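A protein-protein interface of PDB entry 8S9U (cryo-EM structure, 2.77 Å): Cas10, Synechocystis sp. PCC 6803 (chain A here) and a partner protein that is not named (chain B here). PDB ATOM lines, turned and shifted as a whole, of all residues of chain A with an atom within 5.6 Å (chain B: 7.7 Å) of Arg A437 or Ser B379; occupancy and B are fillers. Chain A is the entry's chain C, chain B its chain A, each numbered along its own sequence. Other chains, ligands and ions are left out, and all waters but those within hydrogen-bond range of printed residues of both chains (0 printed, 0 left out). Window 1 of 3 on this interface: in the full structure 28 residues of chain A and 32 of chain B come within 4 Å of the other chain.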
ATOM      1  N   SER A 431      -9.399  -4.728 -27.208  1.00  0.00           N
ATOM      2  CA  SER A 431      -8.336  -3.874 -27.747  1.00  0.00           C
ATOM      3  C   SER A 431      -7.548  -3.042 -26.735  1.00  0.00           C
ATOM      4  O   SER A 431      -6.491  -2.521 -27.103  1.00  0.00           O
ATOM      5  CB  SER A 431      -8.906  -2.950 -28.812  1.00  0.00           C
ATOM      6  OG  SER A 431      -9.568  -3.695 -29.817  1.00  0.00           O
ATOM      7  N   GLY A 432      -8.003  -2.867 -25.498  1.00  0.00           N
ATOM      8  CA  GLY A 432      -7.184  -2.148 -24.528  1.00  0.00           C
ATOM      9  C   GLY A 432      -7.802  -0.915 -23.889  1.00  0.00           C
ATOM     10  O   GLY A 432      -7.116  -0.256 -23.098  1.00  0.00           O
ATOM     11  N   ASP A 434      -7.747   1.911 -23.697  1.00  0.00           N
ATOM     12  CA  ASP A 434      -6.998   3.150 -23.868  1.00  0.00           C
ATOM     13  C   ASP A 434      -6.561   3.271 -25.321  1.00  0.00           C
ATOM     14  O   ASP A 434      -5.982   2.337 -25.883  1.00  0.00           O
ATOM     15  CB  ASP A 434      -5.785   3.192 -22.939  1.00  0.00           C
ATOM     16  CG  ASP A 434      -4.977   4.470 -23.081  1.00  0.00           C
ATOM     17  OD1 ASP A 434      -5.417   5.395 -23.794  1.00  0.00           O
ATOM     18  OD2 ASP A 434      -3.892   4.552 -22.473  1.00  0.00           O
ATOM     19  N   PHE A 435      -6.844   4.431 -25.916  1.00  0.00           N
ATOM     20  CA  PHE A 435      -6.600   4.646 -27.338  1.00  0.00           C
ATOM     21  C   PHE A 435      -5.148   4.423 -27.734  1.00  0.00           C
ATOM     22  O   PHE A 435      -4.873   3.834 -28.784  1.00  0.00           O
ATOM     23  CB  PHE A 435      -7.036   6.052 -27.727  1.00  0.00           C
ATOM     24  CG  PHE A 435      -6.782   6.369 -29.152  1.00  0.00           C
ATOM     25  CD1 PHE A 435      -7.675   5.993 -30.117  1.00  0.00           C
ATOM     26  CD2 PHE A 435      -5.631   7.029 -29.528  1.00  0.00           C
ATOM     27  CE1 PHE A 435      -7.436   6.275 -31.428  1.00  0.00           C
ATOM     28  CE2 PHE A 435      -5.387   7.307 -30.841  1.00  0.00           C
ATOM     29  CZ  PHE A 435      -6.289   6.923 -31.792  1.00  0.00           C
ATOM     30  N   ASP A 436      -4.205   4.895 -26.922  1.00  0.00           N
ATOM     31  CA  ASP A 436      -2.792   4.731 -27.254  1.00  0.00           C
ATOM     32  C   ASP A 436      -2.417   3.256 -27.353  1.00  0.00           C
ATOM     33  O   ASP A 436      -1.727   2.836 -28.288  1.00  0.00           O
ATOM     34  CB  ASP A 436      -1.939   5.452 -26.207  1.00  0.00           C
ATOM     35  CG  ASP A 436      -0.489   5.595 -26.624  1.00  0.00           C
ATOM     36  OD1 ASP A 436      -0.160   5.247 -27.774  1.00  0.00           O
ATOM     37  OD2 ASP A 436       0.328   6.047 -25.794  1.00  0.00           O
ATOM     38  N   ARG A 437      -2.863   2.456 -26.388  1.00  0.00           N
ATOM     39  CA  ARG A 437      -2.677   1.009 -26.442  1.00  0.00           C
ATOM     40  C   ARG A 437      -3.496   0.363 -27.554  1.00  0.00           C
ATOM     41  O   ARG A 437      -3.061  -0.628 -28.148  1.00  0.00           O
ATOM     42  CB  ARG A 437      -3.009   0.377 -25.090  1.00  0.00           C
ATOM     43  CG  ARG A 437      -1.942   0.571 -24.017  1.00  0.00           C
ATOM     44  CD  ARG A 437      -1.818   2.016 -23.568  1.00  0.00           C
ATOM     45  NE  ARG A 437      -0.946   2.150 -22.411  1.00  0.00           N
ATOM     46  CZ  ARG A 437      -0.918   3.212 -21.615  1.00  0.00           C
ATOM     47  NH1 ARG A 437      -1.736   4.229 -21.835  1.00  0.00           N
ATOM     48  NH2 ARG A 437      -0.086   3.245 -20.584  1.00  0.00           N
ATOM     49  N   ILE A 438      -4.689   0.890 -27.837  1.00  0.00           N
ATOM     50  CA  ILE A 438      -5.544   0.312 -28.875  1.00  0.00           C
ATOM     51  C   ILE A 438      -4.844   0.307 -30.225  1.00  0.00           C
ATOM     52  O   ILE A 438      -4.864  -0.698 -30.946  1.00  0.00           O
ATOM     53  CB  ILE A 438      -6.883   1.076 -28.946  1.00  0.00           C
ATOM     54  CG1 ILE A 438      -7.816   0.663 -27.808  1.00  0.00           C
ATOM     55  CG2 ILE A 438      -7.547   0.895 -30.301  1.00  0.00           C
ATOM     56  CD1 ILE A 438      -8.962   1.585 -27.608  1.00  0.00           C
ATOM     57  N   ARG A 439      -4.202   1.415 -30.584  1.00  0.00           N
ATOM     58  CA  ARG A 439      -3.600   1.525 -31.906  1.00  0.00           C
ATOM     59  C   ARG A 439      -2.253   0.821 -32.014  1.00  0.00           C
ATOM     60  O   ARG A 439      -1.871   0.414 -33.113  1.00  0.00           O
ATOM     61  CB  ARG A 439      -3.454   2.996 -32.277  1.00  0.00           C
ATOM     62  CG  ARG A 439      -4.776   3.710 -32.466  1.00  0.00           C
ATOM     63  CD  ARG A 439      -5.471   3.270 -33.740  1.00  0.00           C
ATOM     64  NE  ARG A 439      -6.922   3.402 -33.669  1.00  0.00           N
ATOM     65  CZ  ARG A 439      -7.607   4.387 -34.234  1.00  0.00           C
ATOM     66  NH1 ARG A 439      -8.926   4.418 -34.144  1.00  0.00           N
ATOM     67  NH2 ARG A 439      -6.973   5.346 -34.886  1.00  0.00           N
ATOM     68  N   GLU A 440      -1.517   0.663 -30.914  1.00  0.00           N
ATOM     69  CA  GLU A 440      -0.236  -0.032 -31.000  1.00  0.00           C
ATOM     70  C   GLU A 440      -0.382  -1.543 -31.080  1.00  0.00           C
ATOM     71  O   GLU A 440       0.625  -2.233 -31.257  1.00  0.00           O
ATOM     72  CB  GLU A 440       0.663   0.337 -29.817  1.00  0.00           C
ATOM     73  CG  GLU A 440       0.104  -0.013 -28.454  1.00  0.00           C
ATOM     74  CD  GLU A 440       0.971  -1.013 -27.714  1.00  0.00           C
ATOM     75  OE1 GLU A 440       2.097  -1.284 -28.186  1.00  0.00           O
ATOM     76  OE2 GLU A 440       0.532  -1.528 -26.664  1.00  0.00           O
ATOM     77  N   LYS A 441      -1.594  -2.075 -30.960  1.00  0.00           N
ATOM     78  CA  LYS A 441      -1.822  -3.501 -31.141  1.00  0.00           C
ATOM     79  C   LYS A 441      -2.218  -3.800 -32.572  1.00  0.00           C
ATOM     80  O   LYS A 441      -2.451  -4.960 -32.922  1.00  0.00           O
ATOM     81  CB  LYS A 441      -2.892  -4.008 -30.175  1.00  0.00           C
ATOM     82  CG  LYS A 441      -2.659  -3.588 -28.749  1.00  0.00           C
ATOM     83  CD  LYS A 441      -2.919  -4.723 -27.792  1.00  0.00           C
ATOM     84  CE  LYS A 441      -4.344  -5.199 -27.887  1.00  0.00           C
ATOM     85  NZ  LYS A 441      -4.699  -6.060 -26.732  1.00  0.00           N
ATOM     86  N   MET B  20      -8.663  -8.394 -22.251  1.00  0.00           N
ATOM     87  CA  MET B  20      -8.347  -7.752 -23.514  1.00  0.00           C
ATOM     88  C   MET B  20      -7.649  -8.774 -24.402  1.00  0.00           C
ATOM     89  O   MET B  20      -7.178  -9.809 -23.931  1.00  0.00           O
ATOM     90  CB  MET B  20      -7.488  -6.489 -23.348  1.00  0.00           C
ATOM     91  CG  MET B  20      -6.008  -6.721 -23.265  1.00  0.00           C
ATOM     92  SD  MET B  20      -5.073  -5.227 -22.895  1.00  0.00           S
ATOM     93  CE  MET B  20      -6.200  -4.359 -21.817  1.00  0.00           C
ATOM     94  N   GLY B  21      -7.612  -8.486 -25.704  1.00  0.00           N
ATOM     95  CA  GLY B  21      -6.990  -9.384 -26.652  1.00  0.00           C
ATOM     96  C   GLY B  21      -6.196  -8.639 -27.706  1.00  0.00           C
ATOM     97  O   GLY B  21      -6.449  -7.471 -28.002  1.00  0.00           O
ATOM     98  N   VAL B 258       3.390   1.269  -8.342  1.00  0.00           N
ATOM     99  CA  VAL B 258       3.035   1.959  -7.113  1.00  0.00           C
ATOM    100  C   VAL B 258       1.777   2.769  -7.357  1.00  0.00           C
ATOM    101  O   VAL B 258       1.730   3.587  -8.278  1.00  0.00           O
ATOM    102  CB  VAL B 258       4.179   2.855  -6.609  1.00  0.00           C
ATOM    103  CG1 VAL B 258       3.876   3.355  -5.237  1.00  0.00           C
ATOM    104  CG2 VAL B 258       5.460   2.076  -6.574  1.00  0.00           C
ATOM    105  N   GLU B 270      -7.226   6.710  -9.548  1.00  0.00           N
ATOM    106  CA  GLU B 270      -6.229   7.390 -10.354  1.00  0.00           C
ATOM    107  C   GLU B 270      -4.994   7.706  -9.525  1.00  0.00           C
ATOM    108  O   GLU B 270      -5.060   7.840  -8.304  1.00  0.00           O
ATOM    109  CB  GLU B 270      -6.819   8.668 -10.932  1.00  0.00           C
ATOM    110  CG  GLU B 270      -7.986   8.407 -11.848  1.00  0.00           C
ATOM    111  CD  GLU B 270      -8.240   9.545 -12.796  1.00  0.00           C
ATOM    112  OE1 GLU B 270      -8.002  10.707 -12.404  1.00  0.00           O
ATOM    113  OE2 GLU B 270      -8.668   9.282 -13.938  1.00  0.00           O
ATOM    114  N   CYS B 271      -3.861   7.837 -10.203  1.00  0.00           N
ATOM    115  CA  CYS B 271      -2.563   7.842  -9.549  1.00  0.00           C
ATOM    116  C   CYS B 271      -1.877   9.177  -9.776  1.00  0.00           C
ATOM    117  O   CYS B 271      -2.012   9.785 -10.839  1.00  0.00           O
ATOM    118  CB  CYS B 271      -1.685   6.705 -10.076  1.00  0.00           C
ATOM    119  SG  CYS B 271      -0.205   6.377  -9.128  1.00  0.00           S
ATOM    120  N   LEU B 272      -1.163   9.637  -8.758  1.00  0.00           N
ATOM    121  CA  LEU B 272      -0.204  10.716  -8.895  1.00  0.00           C
ATOM    122  C   LEU B 272       0.992  10.276  -9.728  1.00  0.00           C
ATOM    123  O   LEU B 272       1.308   9.091  -9.833  1.00  0.00           O
ATOM    124  CB  LEU B 272       0.266  11.181  -7.525  1.00  0.00           C
ATOM    125  CG  LEU B 272      -0.828  11.663  -6.595  1.00  0.00           C
ATOM    126  CD1 LEU B 272      -0.233  11.990  -5.271  1.00  0.00           C
ATOM    127  CD2 LEU B 272      -1.478  12.873  -7.179  1.00  0.00           C
ATOM    128  N   ASP B 273       1.661  11.253 -10.332  1.00  0.00           N
ATOM    129  CA  ASP B 273       2.934  11.030 -11.002  1.00  0.00           C
ATOM    130  C   ASP B 273       4.109  11.498 -10.157  1.00  0.00           C
ATOM    131  O   ASP B 273       5.158  11.865 -10.688  1.00  0.00           O
ATOM    132  CB  ASP B 273       2.946  11.707 -12.368  1.00  0.00           C
ATOM    133  CG  ASP B 273       2.604  13.161 -12.290  1.00  0.00           C
ATOM    134  OD1 ASP B 273       2.182  13.612 -11.209  1.00  0.00           O
ATOM    135  OD2 ASP B 273       2.745  13.859 -13.314  1.00  0.00           O
ATOM    136  N   LYS B 376       8.899  12.541 -18.186  1.00  0.00           N
ATOM    137  CA  LYS B 376       7.546  12.004 -18.197  1.00  0.00           C
ATOM    138  C   LYS B 376       7.494  10.739 -17.357  1.00  0.00           C
ATOM    139  O   LYS B 376       8.423   9.925 -17.381  1.00  0.00           O
ATOM    140  CB  LYS B 376       7.049  11.684 -19.609  1.00  0.00           C
ATOM    141  CG  LYS B 376       7.733  10.500 -20.262  1.00  0.00           C
ATOM    142  CD  LYS B 376       7.346  10.383 -21.716  1.00  0.00           C
ATOM    143  CE  LYS B 376       5.866  10.095 -21.863  1.00  0.00           C
ATOM    144  NZ  LYS B 376       5.508   9.850 -23.288  1.00  0.00           N
ATOM    145  N   ILE B 377       6.420  10.602 -16.589  1.00  0.00           N
ATOM    146  CA  ILE B 377       6.213   9.459 -15.715  1.00  0.00           C
ATOM    147  C   ILE B 377       5.277   8.495 -16.423  1.00  0.00           C
ATOM    148  O   ILE B 377       4.144   8.850 -16.762  1.00  0.00           O
ATOM    149  CB  ILE B 377       5.649   9.879 -14.352  1.00  0.00           C
ATOM    150  CG1 ILE B 377       6.656  10.732 -13.595  1.00  0.00           C
ATOM    151  CG2 ILE B 377       5.332   8.667 -13.530  1.00  0.00           C
ATOM    152  CD1 ILE B 377       6.613  12.189 -13.940  1.00  0.00           C
ATOM    153  N   ASN B 378       5.764   7.287 -16.667  1.00  0.00           N
ATOM    154  CA  ASN B 378       4.972   6.215 -17.246  1.00  0.00           C
ATOM    155  C   ASN B 378       4.055   5.591 -16.205  1.00  0.00           C
ATOM    156  O   ASN B 378       4.494   5.248 -15.108  1.00  0.00           O
ATOM    157  CB  ASN B 378       5.892   5.159 -17.839  1.00  0.00           C
ATOM    158  CG  ASN B 378       6.793   5.717 -18.900  1.00  0.00           C
ATOM    159  OD1 ASN B 378       6.331   6.275 -19.888  1.00  0.00           O
ATOM    160  ND2 ASN B 378       8.093   5.586 -18.697  1.00  0.00           N
ATOM    161  N   SER B 379       2.780   5.454 -16.546  1.00  0.00           N
ATOM    162  CA  SER B 379       1.798   4.869 -15.652  1.00  0.00           C
ATOM    163  C   SER B 379       0.884   3.955 -16.447  1.00  0.00           C
ATOM    164  O   SER B 379       0.558   4.252 -17.597  1.00  0.00           O
ATOM    165  CB  SER B 379       0.975   5.948 -14.956  1.00  0.00           C
ATOM    166  OG  SER B 379      -0.015   5.376 -14.133  1.00  0.00           O
ATOM    167  N   GLU B 380       0.467   2.846 -15.836  1.00  0.00           N
ATOM    168  CA  GLU B 380      -0.369   1.865 -16.508  1.00  0.00           C
ATOM    169  C   GLU B 380      -1.592   1.583 -15.650  1.00  0.00           C
ATOM    170  O   GLU B 380      -1.529   1.636 -14.424  1.00  0.00           O
ATOM    171  CB  GLU B 380       0.403   0.574 -16.778  1.00  0.00           C
ATOM    172  CG  GLU B 380      -0.327  -0.417 -17.666  1.00  0.00           C
ATOM    173  CD  GLU B 380      -0.783   0.206 -18.987  1.00  0.00           C
ATOM    174  OE1 GLU B 380       0.056   0.341 -19.905  1.00  0.00           O
ATOM    175  OE2 GLU B 380      -1.976   0.561 -19.110  1.00  0.00           O
ATOM    176  N   LEU B 381      -2.711   1.295 -16.305  1.00  0.00           N
ATOM    177  CA  LEU B 381      -3.925   0.850 -15.633  1.00  0.00           C
ATOM    178  C   LEU B 381      -3.931  -0.658 -15.420  1.00  0.00           C
ATOM    179  O   LEU B 381      -3.730  -1.425 -16.363  1.00  0.00           O
ATOM    180  CB  LEU B 381      -5.154   1.272 -16.430  1.00  0.00           C
ATOM    181  CG  LEU B 381      -6.491   1.141 -15.719  1.00  0.00           C
ATOM    182  CD1 LEU B 381      -6.702   2.293 -14.780  1.00  0.00           C
ATOM    183  CD2 LEU B 381      -7.599   1.087 -16.727  1.00  0.00           C
ATOM    184  N   PHE B 382      -4.166  -1.073 -14.179  1.00  0.00           N
ATOM    185  CA  PHE B 382      -4.303  -2.473 -13.806  1.00  0.00           C
ATOM    186  C   PHE B 382      -5.736  -2.737 -13.378  1.00  0.00           C
ATOM    187  O   PHE B 382      -6.315  -1.954 -12.630  1.00  0.00           O
ATOM    188  CB  PHE B 382      -3.367  -2.830 -12.658  1.00  0.00           C
ATOM    189  CG  PHE B 382      -1.921  -2.684 -12.986  1.00  0.00           C
ATOM    190  CD1 PHE B 382      -1.309  -1.459 -12.897  1.00  0.00           C
ATOM    191  CD2 PHE B 382      -1.175  -3.766 -13.367  1.00  0.00           C
ATOM    192  CE1 PHE B 382       0.005  -1.324 -13.194  1.00  0.00           C
ATOM    193  CE2 PHE B 382       0.137  -3.625 -13.661  1.00  0.00           C
ATOM    194  CZ  PHE B 382       0.726  -2.405 -13.577  1.00  0.00           C
ATOM    195  N   TYR B 404      -6.747   0.212 -10.767  1.00  0.00           N
ATOM    196  CA  TYR B 404      -5.747   1.149 -10.273  1.00  0.00           C
ATOM    197  C   TYR B 404      -4.866   1.602 -11.422  1.00  0.00           C
ATOM    198  O   TYR B 404      -4.340   0.767 -12.158  1.00  0.00           O
ATOM    199  CB  TYR B 404      -4.852   0.520  -9.206  1.00  0.00           C
ATOM    200  CG  TYR B 404      -5.516   0.014  -7.958  1.00  0.00           C
ATOM    201  CD1 TYR B 404      -6.640   0.618  -7.449  1.00  0.00           C
ATOM    202  CD2 TYR B 404      -4.987  -1.050  -7.270  1.00  0.00           C
ATOM    203  CE1 TYR B 404      -7.238   0.145  -6.320  1.00  0.00           C
ATOM    204  CE2 TYR B 404      -5.561  -1.511  -6.136  1.00  0.00           C
ATOM    205  CZ  TYR B 404      -6.690  -0.916  -5.664  1.00  0.00           C
ATOM    206  OH  TYR B 404      -7.256  -1.370  -4.500  1.00  0.00           O
ATOM    207  N   GLU B 405      -4.705   2.910 -11.586  1.00  0.00           N
ATOM    208  CA  GLU B 405      -3.505   3.406 -12.243  1.00  0.00           C
ATOM    209  C   GLU B 405      -2.321   3.242 -11.311  1.00  0.00           C
ATOM    210  O   GLU B 405      -2.429   3.476 -10.107  1.00  0.00           O
ATOM    211  CB  GLU B 405      -3.642   4.871 -12.632  1.00  0.00           C
ATOM    212  CG  GLU B 405      -4.597   5.138 -13.745  1.00  0.00           C
ATOM    213  CD  GLU B 405      -4.609   6.594 -14.139  1.00  0.00           C
ATOM    214  OE1 GLU B 405      -4.226   7.439 -13.306  1.00  0.00           O
ATOM    215  OE2 GLU B 405      -4.999   6.895 -15.286  1.00  0.00           O
ATOM    216  N   ALA B 406      -1.174   2.878 -11.865  1.00  0.00           N
ATOM    217  CA  ALA B 406       0.028   2.804 -11.063  1.00  0.00           C
ATOM    218  C   ALA B 406       1.212   3.352 -11.838  1.00  0.00           C
ATOM    219  O   ALA B 406       1.319   3.168 -13.048  1.00  0.00           O
ATOM    220  CB  ALA B 406       0.303   1.367 -10.641  1.00  0.00           C
ATOM    221  N   ILE B 407       2.112   4.012 -11.113  1.00  0.00           N
ATOM    222  CA  ILE B 407       3.455   4.274 -11.609  1.00  0.00           C
ATOM    223  C   ILE B 407       4.157   2.946 -11.811  1.00  0.00           C
ATOM    224  O   ILE B 407       4.394   2.212 -10.848  1.00  0.00           O
ATOM    225  CB  ILE B 407       4.216   5.145 -10.616  1.00  0.00           C
ATOM    226  CG1 ILE B 407       3.558   6.505 -10.483  1.00  0.00           C
ATOM    227  CG2 ILE B 407       5.632   5.316 -11.056  1.00  0.00           C
ATOM    228  CD1 ILE B 407       4.325   7.426  -9.608  1.00  0.00           C
ATOM    229  N   ILE B 408       4.541   2.648 -13.045  1.00  0.00           N
ATOM    230  CA  ILE B 408       5.126   1.348 -13.345  1.00  0.00           C
ATOM    231  C   ILE B 408       6.525   1.219 -12.760  1.00  0.00           C
ATOM    232  O   ILE B 408       7.117   2.202 -12.312  1.00  0.00           O
ATOM    233  CB  ILE B 408       5.114   1.081 -14.859  1.00  0.00           C
ATOM    234  CG1 ILE B 408       6.043   2.031 -15.593  1.00  0.00           C
ATOM    235  CG2 ILE B 408       3.726   1.229 -15.398  1.00  0.00           C
ATOM    236  CD1 ILE B 408       6.240   1.652 -17.019  1.00  0.00           C
ATOM    237  N   GLN B 411      10.846   3.275 -12.722  1.00  0.00           N
ATOM    238  CA  GLN B 411      10.869   4.721 -12.600  1.00  0.00           C
ATOM    239  C   GLN B 411      11.790   5.122 -11.457  1.00  0.00           C
ATOM    240  O   GLN B 411      11.892   4.416 -10.455  1.00  0.00           O
ATOM    241  CB  GLN B 411       9.462   5.231 -12.318  1.00  0.00           C
ATOM    242  CG  GLN B 411       8.398   4.821 -13.315  1.00  0.00           C
ATOM    243  CD  GLN B 411       8.565   5.431 -14.644  1.00  0.00           C
ATOM    244  OE1 GLN B 411       8.718   4.734 -15.633  1.00  0.00           O
ATOM    245  NE2 GLN B 411       8.526   6.743 -14.695  1.00  0.00           N
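Of the printed residues of chain B, Gly A432 touches Met B20. Arg A437 touches just these residues of chain B: Ser B379 and Glu B380. Of the printed residues of chain B, Lys A441 touches Met B20 and Gly B21. Printed residues of chain A within 4 Å of Met B20: Gly A432 and Lys A441. Of the printed residues of chain A, Gly B21 touches Lys A441 (2.6 Å). Val B258 touches none of the printed residues of chain A. Of the printed residues of chain A, Glu B380 touches Arg A437. The nearest residue of chain B that does not touch Arg A437 is Leu B381 (5.4 Å).
Printed residues of chain B that touch a printed residue of chain A: Met B20, Gly B21, Ser B379 and Glu B380. Hydrophobic or aromatic side chains of chain B within 4 Å of the printed part of chain A: Met B20. Among the printed residues, Asp or Glu carboxylates within 4 Å of a Lys or Arg side-chain nitrogen of the other chain: Arg A437 with Glu B380 (3.0 Å).
The backbone NH (N) of Ala B406 sits at hydrogen-bond distance from the backbone carbonyl oxygen (O) of Glu B380, at 2.9 Å. OG of Ser B379 sits at hydrogen-bond distance from O of Ala B406. The guanidinium group of Arg A437 is in salt-bridge range of the side-chain carboxylate of Asp A434, 3.8 Å away.
Among the printed residues, pairs that only touch across the chains: Gly A432 with Met B20 and Lys A441 with Met B20.
O of Ser B379 lies within hydrogen-bond range of NH2 of Arg A437 (3.2 Å). NZ of Lys A441 is in hydrogen-bond range of O of Gly B21. OE1 of Glu B380 is in salt-bridge range of NH2 of Arg A437, at 3.0 Å.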
